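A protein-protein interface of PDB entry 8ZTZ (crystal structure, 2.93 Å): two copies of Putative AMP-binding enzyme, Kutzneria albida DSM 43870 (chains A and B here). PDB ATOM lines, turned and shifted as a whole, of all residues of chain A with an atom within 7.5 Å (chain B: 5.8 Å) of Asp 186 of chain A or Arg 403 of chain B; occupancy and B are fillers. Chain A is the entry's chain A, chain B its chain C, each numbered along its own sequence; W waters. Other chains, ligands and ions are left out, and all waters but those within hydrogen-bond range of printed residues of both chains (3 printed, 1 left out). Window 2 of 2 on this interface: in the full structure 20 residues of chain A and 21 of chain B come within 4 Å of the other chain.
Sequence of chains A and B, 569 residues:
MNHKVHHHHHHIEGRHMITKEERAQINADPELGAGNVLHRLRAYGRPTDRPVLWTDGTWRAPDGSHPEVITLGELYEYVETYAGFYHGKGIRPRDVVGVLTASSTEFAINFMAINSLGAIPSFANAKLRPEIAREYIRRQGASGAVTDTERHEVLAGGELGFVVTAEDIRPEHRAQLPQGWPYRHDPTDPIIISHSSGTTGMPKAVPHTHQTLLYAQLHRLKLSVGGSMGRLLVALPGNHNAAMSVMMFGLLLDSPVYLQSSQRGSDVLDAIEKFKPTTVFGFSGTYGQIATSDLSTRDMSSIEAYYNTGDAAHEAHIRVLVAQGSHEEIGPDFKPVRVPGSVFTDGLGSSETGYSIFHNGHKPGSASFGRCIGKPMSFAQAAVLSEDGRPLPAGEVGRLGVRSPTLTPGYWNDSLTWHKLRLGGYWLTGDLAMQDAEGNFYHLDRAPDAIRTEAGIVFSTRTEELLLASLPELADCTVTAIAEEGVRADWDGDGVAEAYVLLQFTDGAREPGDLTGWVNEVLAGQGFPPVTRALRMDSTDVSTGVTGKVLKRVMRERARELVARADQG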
ATOM      1  N   GLU A  31     -12.215 -18.383   7.308  1.00  0.00           N
ATOM      2  CA  GLU A  31     -11.109 -18.031   8.201  1.00  0.00           C
ATOM      3  C   GLU A  31     -11.063 -16.544   8.551  1.00  0.00           C
ATOM      4  O   GLU A  31     -10.363 -16.166   9.498  1.00  0.00           O
ATOM      5  CB  GLU A  31      -9.760 -18.431   7.579  1.00  0.00           C
ATOM      6  CG  GLU A  31      -9.457 -19.938   7.522  1.00  0.00           C
ATOM      7  CD  GLU A  31      -8.352 -20.300   6.494  1.00  0.00           C
ATOM      8  OE1 GLU A  31      -8.395 -19.842   5.317  1.00  0.00           O
ATOM      9  OE2 GLU A  31      -7.426 -21.051   6.881  1.00  0.00           O
ATOM     10  N   GLY A  35      -8.845 -10.997  13.734  1.00  0.00           N
ATOM     11  CA  GLY A  35      -7.422 -11.255  13.805  1.00  0.00           C
ATOM     12  C   GLY A  35      -6.661 -11.407  12.497  1.00  0.00           C
ATOM     13  O   GLY A  35      -5.448 -11.602  12.552  1.00  0.00           O
ATOM     14  N   ARG A  94      -1.102 -15.435  23.028  1.00  0.00           N
ATOM     15  CA  ARG A  94      -1.884 -15.225  24.250  1.00  0.00           C
ATOM     16  C   ARG A  94      -1.160 -14.350  25.268  1.00  0.00           C
ATOM     17  O   ARG A  94      -1.635 -14.213  26.397  1.00  0.00           O
ATOM     18  CB  ARG A  94      -2.305 -16.533  24.925  1.00  0.00           C
ATOM     19  CG  ARG A  94      -2.826 -17.578  23.975  1.00  0.00           C
ATOM     20  CD  ARG A  94      -4.263 -17.361  23.570  1.00  0.00           C
ATOM     21  NE  ARG A  94      -4.814 -18.569  22.962  1.00  0.00           N
ATOM     22  CZ  ARG A  94      -4.948 -18.723  21.653  1.00  0.00           C
ATOM     23  NH1 ARG A  94      -4.662 -17.740  20.816  1.00  0.00           N
ATOM     24  NH2 ARG A  94      -5.376 -19.886  21.171  1.00  0.00           N
ATOM     25  N   TYR A 183      -0.512 -15.679  12.559  1.00  0.00           N
ATOM     26  CA  TYR A 183      -1.195 -16.607  13.444  1.00  0.00           C
ATOM     27  C   TYR A 183      -2.503 -17.029  12.802  1.00  0.00           C
ATOM     28  O   TYR A 183      -3.068 -16.311  11.976  1.00  0.00           O
ATOM     29  CB  TYR A 183      -1.432 -15.949  14.815  1.00  0.00           C
ATOM     30  CG  TYR A 183      -1.921 -16.879  15.897  1.00  0.00           C
ATOM     31  CD1 TYR A 183      -1.051 -17.713  16.555  1.00  0.00           C
ATOM     32  CD2 TYR A 183      -3.257 -16.904  16.275  1.00  0.00           C
ATOM     33  CE1 TYR A 183      -1.494 -18.573  17.548  1.00  0.00           C
ATOM     34  CE2 TYR A 183      -3.705 -17.753  17.262  1.00  0.00           C
ATOM     35  CZ  TYR A 183      -2.817 -18.589  17.896  1.00  0.00           C
ATOM     36  OH  TYR A 183      -3.236 -19.443  18.887  1.00  0.00           O
ATOM     37  N   ARG A 184      -2.970 -18.216  13.159  1.00  0.00           N
ATOM     38  CA  ARG A 184      -4.231 -18.729  12.628  1.00  0.00           C
ATOM     39  C   ARG A 184      -5.250 -18.750  13.768  1.00  0.00           C
ATOM     40  O   ARG A 184      -5.330 -19.715  14.535  1.00  0.00           O
ATOM     41  CB  ARG A 184      -4.032 -20.092  12.016  1.00  0.00           C
ATOM     42  CG  ARG A 184      -5.304 -20.773  11.615  1.00  0.00           C
ATOM     43  CD  ARG A 184      -5.015 -22.241  11.329  1.00  0.00           C
ATOM     44  NE  ARG A 184      -5.541 -23.134  12.356  1.00  0.00           N
ATOM     45  CZ  ARG A 184      -6.755 -23.663  12.320  1.00  0.00           C
ATOM     46  NH1 ARG A 184      -7.599 -23.388  11.332  1.00  0.00           N
ATOM     47  NH2 ARG A 184      -7.131 -24.486  13.296  1.00  0.00           N
ATOM     48  N   HIS A 185      -6.026 -17.669  13.887  1.00  0.00           N
ATOM     49  CA  HIS A 185      -6.977 -17.563  14.983  1.00  0.00           C
ATOM     50  C   HIS A 185      -8.104 -18.558  14.797  1.00  0.00           C
ATOM     51  O   HIS A 185      -8.633 -18.710  13.685  1.00  0.00           O
ATOM     52  CB  HIS A 185      -7.568 -16.162  15.070  1.00  0.00           C
ATOM     53  CG  HIS A 185      -6.577 -15.106  15.430  1.00  0.00           C
ATOM     54  ND1 HIS A 185      -5.964 -14.313  14.488  1.00  0.00           N
ATOM     55  CD2 HIS A 185      -6.096 -14.708  16.628  1.00  0.00           C
ATOM     56  CE1 HIS A 185      -5.141 -13.473  15.090  1.00  0.00           C
ATOM     57  NE2 HIS A 185      -5.202 -13.694  16.390  1.00  0.00           N
ATOM     58  N   ASP A 186      -8.434 -19.262  15.884  1.00  0.00           N
ATOM     59  CA  ASP A 186      -9.763 -19.810  16.049  1.00  0.00           C
ATOM     60  C   ASP A 186     -10.733 -18.657  16.303  1.00  0.00           C
ATOM     61  O   ASP A 186     -10.338 -17.616  16.847  1.00  0.00           O
ATOM     62  CB  ASP A 186      -9.808 -20.787  17.218  1.00  0.00           C
ATOM     63  CG  ASP A 186     -11.137 -21.516  17.318  1.00  0.00           C
ATOM     64  OD1 ASP A 186     -11.332 -22.496  16.563  1.00  0.00           O
ATOM     65  OD2 ASP A 186     -11.993 -21.109  18.133  1.00  0.00           O
ATOM     66  N   PRO A 187     -11.992 -18.800  15.883  1.00  0.00           N
ATOM     67  CA  PRO A 187     -13.010 -17.778  16.177  1.00  0.00           C
ATOM     68  C   PRO A 187     -13.002 -17.255  17.607  1.00  0.00           C
ATOM     69  O   PRO A 187     -13.218 -16.064  17.846  1.00  0.00           O
ATOM     70  CB  PRO A 187     -14.319 -18.523  15.883  1.00  0.00           C
ATOM     71  CG  PRO A 187     -13.959 -19.464  14.806  1.00  0.00           C
ATOM     72  CD  PRO A 187     -12.507 -19.842  14.984  1.00  0.00           C
ATOM     73  N   THR A 188     -12.758 -18.130  18.567  1.00  0.00           N
ATOM     74  CA  THR A 188     -12.872 -17.784  19.963  1.00  0.00           C
ATOM     75  C   THR A 188     -11.588 -17.187  20.521  1.00  0.00           C
ATOM     76  O   THR A 188     -11.502 -16.951  21.732  1.00  0.00           O
ATOM     77  CB  THR A 188     -13.267 -19.025  20.742  1.00  0.00           C
ATOM     78  OG1 THR A 188     -12.407 -20.092  20.347  1.00  0.00           O
ATOM     79  CG2 THR A 188     -14.673 -19.426  20.415  1.00  0.00           C
ATOM     80  N   ASP A 189     -10.604 -16.904  19.676  1.00  0.00           N
ATOM     81  CA  ASP A 189      -9.346 -16.430  20.246  1.00  0.00           C
ATOM     82  C   ASP A 189      -9.363 -14.915  20.428  1.00  0.00           C
ATOM     83  O   ASP A 189      -9.679 -14.183  19.476  1.00  0.00           O
ATOM     84  CB  ASP A 189      -8.173 -16.825  19.372  1.00  0.00           C
ATOM     85  CG  ASP A 189      -7.780 -18.252  19.571  1.00  0.00           C
ATOM     86  OD1 ASP A 189      -8.075 -18.770  20.668  1.00  0.00           O
ATOM     87  OD2 ASP A 189      -7.198 -18.853  18.640  1.00  0.00           O
ATOM     88  N   PRO A 190      -9.018 -14.435  21.629  1.00  0.00           N
ATOM     89  CA  PRO A 190      -8.958 -12.985  21.878  1.00  0.00           C
ATOM     90  C   PRO A 190      -8.016 -12.280  20.917  1.00  0.00           C
ATOM     91  O   PRO A 190      -6.908 -12.745  20.645  1.00  0.00           O
ATOM     92  CB  PRO A 190      -8.439 -12.892  23.320  1.00  0.00           C
ATOM     93  CG  PRO A 190      -8.760 -14.214  23.939  1.00  0.00           C
ATOM     94  CD  PRO A 190      -8.727 -15.232  22.836  1.00  0.00           C
ATOM     95  N   ILE A 191      -8.463 -11.135  20.406  1.00  0.00           N
ATOM     96  CA  ILE A 191      -7.663 -10.330  19.493  1.00  0.00           C
ATOM     97  C   ILE A 191      -7.601  -8.864  19.897  1.00  0.00           C
ATOM     98  O   ILE A 191      -7.013  -8.061  19.175  1.00  0.00           O
ATOM     99  CB  ILE A 191      -8.159 -10.467  18.038  1.00  0.00           C
ATOM    100  CG1 ILE A 191      -9.654 -10.175  17.929  1.00  0.00           C
ATOM    101  CG2 ILE A 191      -7.909 -11.864  17.545  1.00  0.00           C
ATOM    102  CD1 ILE A 191      -9.990  -8.723  17.798  1.00  0.00           C
ATOM    103  N   THR A 209     -13.031 -11.269  20.509  1.00  0.00           N
ATOM    104  CA  THR A 209     -12.416 -12.393  19.829  1.00  0.00           C
ATOM    105  C   THR A 209     -12.397 -12.181  18.322  1.00  0.00           C
ATOM    106  O   THR A 209     -13.035 -11.275  17.770  1.00  0.00           O
ATOM    107  CB  THR A 209     -13.156 -13.680  20.162  1.00  0.00           C
ATOM    108  OG1 THR A 209     -14.515 -13.532  19.734  1.00  0.00           O
ATOM    109  CG2 THR A 209     -13.093 -13.933  21.674  1.00  0.00           C
ATOM    110  N   HIS A 210     -11.617 -13.037  17.669  1.00  0.00           N
ATOM    111  CA  HIS A 210     -11.553 -13.104  16.219  1.00  0.00           C
ATOM    112  C   HIS A 210     -12.937 -13.032  15.576  1.00  0.00           C
ATOM    113  O   HIS A 210     -13.169 -12.285  14.619  1.00  0.00           O
ATOM    114  CB  HIS A 210     -10.839 -14.406  15.870  1.00  0.00           C
ATOM    115  CG  HIS A 210     -10.658 -14.627  14.413  1.00  0.00           C
ATOM    116  ND1 HIS A 210     -10.082 -13.693  13.585  1.00  0.00           N
ATOM    117  CD2 HIS A 210     -10.972 -15.685  13.636  1.00  0.00           C
ATOM    118  CE1 HIS A 210     -10.032 -14.176  12.359  1.00  0.00           C
ATOM    119  NE2 HIS A 210     -10.586 -15.372  12.358  1.00  0.00           N
ATOM    120  N   GLN A 211     -13.881 -13.772  16.131  1.00  0.00           N
ATOM    121  CA  GLN A 211     -15.236 -13.778  15.602  1.00  0.00           C
ATOM    122  C   GLN A 211     -16.030 -12.526  15.995  1.00  0.00           C
ATOM    123  O   GLN A 211     -16.633 -11.882  15.128  1.00  0.00           O
ATOM    124  CB  GLN A 211     -15.946 -15.039  16.073  1.00  0.00           C
ATOM    125  CG  GLN A 211     -17.395 -15.132  15.677  1.00  0.00           C
ATOM    126  CD  GLN A 211     -17.980 -16.490  16.033  1.00  0.00           C
ATOM    127  OE1 GLN A 211     -17.669 -17.071  17.103  1.00  0.00           O
ATOM    128  NE2 GLN A 211     -18.811 -17.019  15.132  1.00  0.00           N
ATOM    129  N   PHE B 379     -20.976 -36.524  23.426  1.00  0.00           N
ATOM    130  CA  PHE B 379     -21.280 -35.095  23.479  1.00  0.00           C
ATOM    131  C   PHE B 379     -20.048 -34.204  23.391  1.00  0.00           C
ATOM    132  O   PHE B 379     -20.196 -33.002  23.141  1.00  0.00           O
ATOM    133  CB  PHE B 379     -22.048 -34.744  24.748  1.00  0.00           C
ATOM    134  CG  PHE B 379     -21.401 -35.221  25.995  1.00  0.00           C
ATOM    135  CD1 PHE B 379     -20.193 -34.699  26.409  1.00  0.00           C
ATOM    136  CD2 PHE B 379     -22.014 -36.183  26.772  1.00  0.00           C
ATOM    137  CE1 PHE B 379     -19.595 -35.143  27.559  1.00  0.00           C
ATOM    138  CE2 PHE B 379     -21.433 -36.626  27.927  1.00  0.00           C
ATOM    139  CZ  PHE B 379     -20.218 -36.109  28.327  1.00  0.00           C
ATOM    140  N   ALA B 380     -18.857 -34.750  23.598  1.00  0.00           N
ATOM    141  CA  ALA B 380     -17.624 -33.993  23.504  1.00  0.00           C
ATOM    142  C   ALA B 380     -16.949 -34.233  22.161  1.00  0.00           C
ATOM    143  O   ALA B 380     -17.209 -35.222  21.474  1.00  0.00           O
ATOM    144  CB  ALA B 380     -16.682 -34.380  24.642  1.00  0.00           C
ATOM    145  N   GLN B 381     -16.076 -33.304  21.784  1.00  0.00           N
ATOM    146  CA  GLN B 381     -15.221 -33.447  20.615  1.00  0.00           C
ATOM    147  C   GLN B 381     -13.784 -33.400  21.106  1.00  0.00           C
ATOM    148  O   GLN B 381     -13.398 -32.450  21.794  1.00  0.00           O
ATOM    149  CB  GLN B 381     -15.480 -32.336  19.589  1.00  0.00           C
ATOM    150  CG  GLN B 381     -16.940 -32.221  19.087  1.00  0.00           C
ATOM    151  CD  GLN B 381     -17.853 -31.316  19.973  1.00  0.00           C
ATOM    152  OE1 GLN B 381     -18.805 -31.795  20.620  1.00  0.00           O
ATOM    153  NE2 GLN B 381     -17.571 -30.003  19.978  1.00  0.00           N
ATOM    154  N   ALA B 382     -12.997 -34.419  20.777  1.00  0.00           N
ATOM    155  CA  ALA B 382     -11.588 -34.431  21.132  1.00  0.00           C
ATOM    156  C   ALA B 382     -10.737 -34.540  19.874  1.00  0.00           C
ATOM    157  O   ALA B 382     -11.189 -35.020  18.837  1.00  0.00           O
ATOM    158  CB  ALA B 382     -11.256 -35.570  22.103  1.00  0.00           C
ATOM    159  N   GLY B 401      -6.777 -32.067  22.735  1.00  0.00           N
ATOM    160  CA  GLY B 401      -7.725 -30.981  22.911  1.00  0.00           C
ATOM    161  C   GLY B 401      -9.122 -31.537  23.108  1.00  0.00           C
ATOM    162  O   GLY B 401      -9.435 -32.636  22.649  1.00  0.00           O
ATOM    163  N   VAL B 402      -9.964 -30.773  23.803  1.00  0.00           N
ATOM    164  CA  VAL B 402     -11.306 -31.223  24.167  1.00  0.00           C
ATOM    165  C   VAL B 402     -12.282 -30.066  24.050  1.00  0.00           C
ATOM    166  O   VAL B 402     -12.025 -28.985  24.583  1.00  0.00           O
ATOM    167  CB  VAL B 402     -11.338 -31.787  25.594  1.00  0.00           C
ATOM    168  CG1 VAL B 402     -12.763 -31.933  26.050  1.00  0.00           C
ATOM    169  CG2 VAL B 402     -10.587 -33.113  25.652  1.00  0.00           C
ATOM    170  N   ARG B 403     -13.383 -30.278  23.343  1.00  0.00           N
ATOM    171  CA  ARG B 403     -14.535 -29.388  23.381  1.00  0.00           C
ATOM    172  C   ARG B 403     -15.695 -30.127  24.023  1.00  0.00           C
ATOM    173  O   ARG B 403     -15.944 -31.295  23.697  1.00  0.00           O
ATOM    174  CB  ARG B 403     -14.960 -28.940  21.987  1.00  0.00           C
ATOM    175  CG  ARG B 403     -13.890 -28.277  21.178  1.00  0.00           C
ATOM    176  CD  ARG B 403     -14.414 -27.985  19.809  1.00  0.00           C
ATOM    177  NE  ARG B 403     -13.529 -27.104  19.066  1.00  0.00           N
ATOM    178  CZ  ARG B 403     -13.831 -26.567  17.890  1.00  0.00           C
ATOM    179  NH1 ARG B 403     -14.984 -26.831  17.286  1.00  0.00           N
ATOM    180  NH2 ARG B 403     -12.958 -25.739  17.307  1.00  0.00           N
ATOM    181  N   SER B 404     -16.418 -29.458  24.927  1.00  0.00           N
ATOM    182  CA  SER B 404     -17.553 -30.176  25.486  1.00  0.00           C
ATOM    183  C   SER B 404     -18.561 -29.249  26.133  1.00  0.00           C
ATOM    184  O   SER B 404     -18.169 -28.264  26.763  1.00  0.00           O
ATOM    185  CB  SER B 404     -17.079 -31.207  26.507  1.00  0.00           C
ATOM    186  OG  SER B 404     -18.161 -31.798  27.189  1.00  0.00           O
ATOM    187  N   PRO B 405     -19.832 -29.540  26.031  1.00  0.00           N
ATOM    188  CA  PRO B 405     -20.843 -28.780  26.771  1.00  0.00           C
ATOM    189  C   PRO B 405     -20.712 -28.908  28.280  1.00  0.00           C
ATOM    190  O   PRO B 405     -21.544 -28.401  29.035  1.00  0.00           O
ATOM    191  CB  PRO B 405     -22.149 -29.412  26.279  1.00  0.00           C
ATOM    192  CG  PRO B 405     -21.762 -30.760  25.919  1.00  0.00           C
ATOM    193  CD  PRO B 405     -20.448 -30.617  25.257  1.00  0.00           C
ATOM    194  N   LEU B 407     -17.577 -28.259  29.584  1.00  0.00           N
ATOM    195  CA  LEU B 407     -16.403 -27.458  29.875  1.00  0.00           C
ATOM    196  C   LEU B 407     -16.778 -26.213  30.673  1.00  0.00           C
ATOM    197  O   LEU B 407     -17.765 -25.537  30.374  1.00  0.00           O
ATOM    198  CB  LEU B 407     -15.724 -27.057  28.576  1.00  0.00           C
ATOM    199  CG  LEU B 407     -14.254 -26.801  28.794  1.00  0.00           C
ATOM    200  CD1 LEU B 407     -13.641 -27.990  29.516  1.00  0.00           C
ATOM    201  CD2 LEU B 407     -13.602 -26.587  27.486  1.00  0.00           C
ATOM    202  N   ARG B 422      -5.728 -22.705  25.809  1.00  0.00           N
ATOM    203  CA  ARG B 422      -6.658 -23.002  24.740  1.00  0.00           C
ATOM    204  C   ARG B 422      -5.929 -22.976  23.406  1.00  0.00           C
ATOM    205  O   ARG B 422      -4.928 -22.271  23.242  1.00  0.00           O
ATOM    206  CB  ARG B 422      -7.813 -22.031  24.759  1.00  0.00           C
ATOM    207  CG  ARG B 422      -8.813 -22.340  25.840  1.00  0.00           C
ATOM    208  CD  ARG B 422      -9.870 -21.241  25.995  1.00  0.00           C
ATOM    209  NE  ARG B 422     -10.279 -20.701  24.702  1.00  0.00           N
ATOM    210  CZ  ARG B 422     -11.279 -21.172  23.981  1.00  0.00           C
ATOM    211  NH1 ARG B 422     -12.044 -22.155  24.426  1.00  0.00           N
ATOM    212  NH2 ARG B 422     -11.507 -20.653  22.783  1.00  0.00           N
ATOM    213  N   LEU B 423      -6.430 -23.773  22.463  1.00  0.00           N
ATOM    214  CA  LEU B 423      -5.767 -23.936  21.181  1.00  0.00           C
ATOM    215  C   LEU B 423      -6.799 -24.352  20.145  1.00  0.00           C
ATOM    216  O   LEU B 423      -7.516 -25.337  20.359  1.00  0.00           O
ATOM    217  CB  LEU B 423      -4.661 -24.977  21.266  1.00  0.00           C
ATOM    218  CG  LEU B 423      -3.788 -25.004  20.017  1.00  0.00           C
ATOM    219  CD1 LEU B 423      -3.365 -23.582  19.614  1.00  0.00           C
ATOM    220  CD2 LEU B 423      -2.587 -25.875  20.296  1.00  0.00           C
ATOM    221  N   GLY B 424      -6.866 -23.605  19.040  1.00  0.00           N
ATOM    222  CA  GLY B 424      -7.804 -23.866  17.965  1.00  0.00           C
ATOM    223  C   GLY B 424      -9.216 -24.166  18.418  1.00  0.00           C
ATOM    224  O   GLY B 424      -9.903 -25.019  17.843  1.00  0.00           O
ATOM    225  N   GLY B 425      -9.660 -23.479  19.464  1.00  0.00           N
ATOM    226  CA  GLY B 425     -10.982 -23.633  19.986  1.00  0.00           C
ATOM    227  C   GLY B 425     -11.140 -24.731  21.000  1.00  0.00           C
ATOM    228  O   GLY B 425     -12.220 -24.842  21.590  1.00  0.00           O
ATOM    229  N   TYR B 426     -10.115 -25.547  21.225  1.00  0.00           N
ATOM    230  CA  TYR B 426     -10.187 -26.613  22.221  1.00  0.00           C
ATOM    231  C   TYR B 426      -9.525 -26.186  23.531  1.00  0.00           C
ATOM    232  O   TYR B 426      -8.688 -25.274  23.572  1.00  0.00           O
ATOM    233  CB  TYR B 426      -9.519 -27.913  21.726  1.00  0.00           C
ATOM    234  CG  TYR B 426     -10.073 -28.482  20.436  1.00  0.00           C
ATOM    235  CD1 TYR B 426      -9.742 -27.914  19.210  1.00  0.00           C
ATOM    236  CD2 TYR B 426     -10.904 -29.599  20.433  1.00  0.00           C
ATOM    237  CE1 TYR B 426     -10.234 -28.417  18.034  1.00  0.00           C
ATOM    238  CE2 TYR B 426     -11.393 -30.110  19.255  1.00  0.00           C
ATOM    239  CZ  TYR B 426     -11.053 -29.513  18.059  1.00  0.00           C
ATOM    240  OH  TYR B 426     -11.537 -29.996  16.867  1.00  0.00           O
ATOM    241  N   TRP B 427      -9.900 -26.879  24.610  1.00  0.00           N
ATOM    242  CA  TRP B 427      -9.160 -26.776  25.856  1.00  0.00           C
ATOM    243  C   TRP B 427      -8.046 -27.818  25.853  1.00  0.00           C
ATOM    244  O   TRP B 427      -8.240 -28.947  25.400  1.00  0.00           O
ATOM    245  CB  TRP B 427     -10.082 -26.966  27.061  1.00  0.00           C
ATOM    246  CG  TRP B 427      -9.347 -26.853  28.345  1.00  0.00           C
ATOM    247  CD1 TRP B 427      -8.828 -25.715  28.906  1.00  0.00           C
ATOM    248  CD2 TRP B 427      -9.011 -27.917  29.241  1.00  0.00           C
ATOM    249  NE1 TRP B 427      -8.212 -26.008  30.104  1.00  0.00           N
ATOM    250  CE2 TRP B 427      -8.308 -27.354  30.322  1.00  0.00           C
ATOM    251  CE3 TRP B 427      -9.249 -29.287  29.239  1.00  0.00           C
ATOM    252  CZ2 TRP B 427      -7.849 -28.109  31.369  1.00  0.00           C
ATOM    253  CZ3 TRP B 427      -8.785 -30.031  30.283  1.00  0.00           C
ATOM    254  CH2 TRP B 427      -8.094 -29.447  31.329  1.00  0.00           C
HETATM  255  O   HOH W   1      -8.568 -19.330  23.129  1.00  0.00           O
HETATM  256  O   HOH W   2      -5.591 -20.909  18.441  1.00  0.00           O
HETATM  257  O   HOH W   3     -13.980 -23.889  15.156  1.00  0.00           O
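NH2 of Arg 94 of chain A is in hydrogen-bond range of O of Arg 422 of chain B, at 3.2 Å.
NH2 of Arg 403 of chain B is in salt-bridge range of OD1 of Asp 186 of chain A, at 3.7 Å.
OD1 of Asp 186 of chain A lies close to N of Gly 425 of chain B, 3.5 Å away.
The side-chain hydroxyl of Thr 188 of chain A lies within hydrogen-bond range of the guanidinium group of Arg 422 of chain B (2.7 Å).
The backbone carbonyl oxygen (O) of Gly 424 of chain B sits close to the side-chain carboxylate (OD1) of Asp 186 of chain A (3.2 Å).
The guanidinium group of Arg 94 of chain A lies within hydrogen-bond range of the side-chain hydroxyl of Tyr 183 of chain A, 2.9 Å away.
The guanidinium group (NH2) of Arg 94 of chain A lies within salt-bridge range of the side-chain carboxylate (OD1) of Asp 189 of chain A, at 3.0 Å.
The side-chain carboxylate of Asp 186 of chain A lies within hydrogen-bond range of the side-chain hydroxyl of Thr 188 of chain A (2.5 Å).
The backbone NH of Asp 186 of chain A is in hydrogen-bond range of the side-chain carboxylate of Asp 189 of chain A (3.0 Å).
N of Arg 403 of chain B lies within hydrogen-bond range of O of Gln 381 of chain B.
O of Gly 424 of chain B is in hydrogen-bond range of NH2 of Arg 403 of chain B (3.2 Å).
Among the printed residues, merely in contact across the chains: Thr 188 of chain A with Gly 425 of chain B (3.8 Å).
Of the printed residues of chain B, Arg 94 of chain A touches Arg 422 (3.2 Å).
Asp 186 of chain A touches just these residues of chain B: Arg 403 (3.7 Å), Gly 424 (3.2 Å) and Gly 425 (3.3 Å).
Of the printed residues of chain B, Thr 188 of chain A touches Arg 422 and Gly 425.
Of the printed residues of chain A, Arg 422 of chain B touches Arg 94 (3.2 Å) and Thr 188 (2.7 Å).
Of the printed residues of chain A, Gly 424 of chain B touches Asp 186 (3.2 Å).
Of the printed residues of chain A, Gly 425 of chain B touches Asp 186 and Thr 188.
Trp 427 of chain B touches none of the printed residues of chain A.
The nearest residue of chain B that does not touch Asp 186 of chain A is Arg 422 of chain B (4.7 Å).
The nearest residue of chain A that does not touch Arg 403 of chain B is Pro 187 of chain A (6.4 Å).
Of the 15 printed residues of chain A, 3 touch a printed residue of chain B.
Printed residues of chain A that touch a printed residue of chain B: Arg 94, Asp 186 and Thr 188.
Printed residues of chain B that touch a printed residue of chain A: Arg 403, Arg 422, Gly 424 and Gly 425.
Among the printed residues, Asp or Glu carboxylates within 4 Å of a Lys or Arg side-chain nitrogen of the other chain: Asp 186 of chain A with Arg 403 of chain B (3.7 Å).
No position is printed for both chains.
Of the 6 pairs that touch across the chains among the printed residues, none has its exchanged pair printed and touching as well.
Water W1 lies within hydrogen-bond range of OD1 of Asp 189 of chain A (2.6 Å) and NE of Arg 422 of chain B (2.7 Å).
Water W2 lies within hydrogen-bond range of OD2 of Asp 189 of chain A (2.6 Å), OH of Tyr 183 of chain A (2.8 Å), NH2 of Arg 94 of chain A (2.9 Å) and N of Gly 424 of chain B (3.0 Å).
Water W3 lies within hydrogen-bond range of NH2 of Arg 403 of chain B (3.0 Å) and OD1 of Asp 186 of chain A (3.3 Å).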
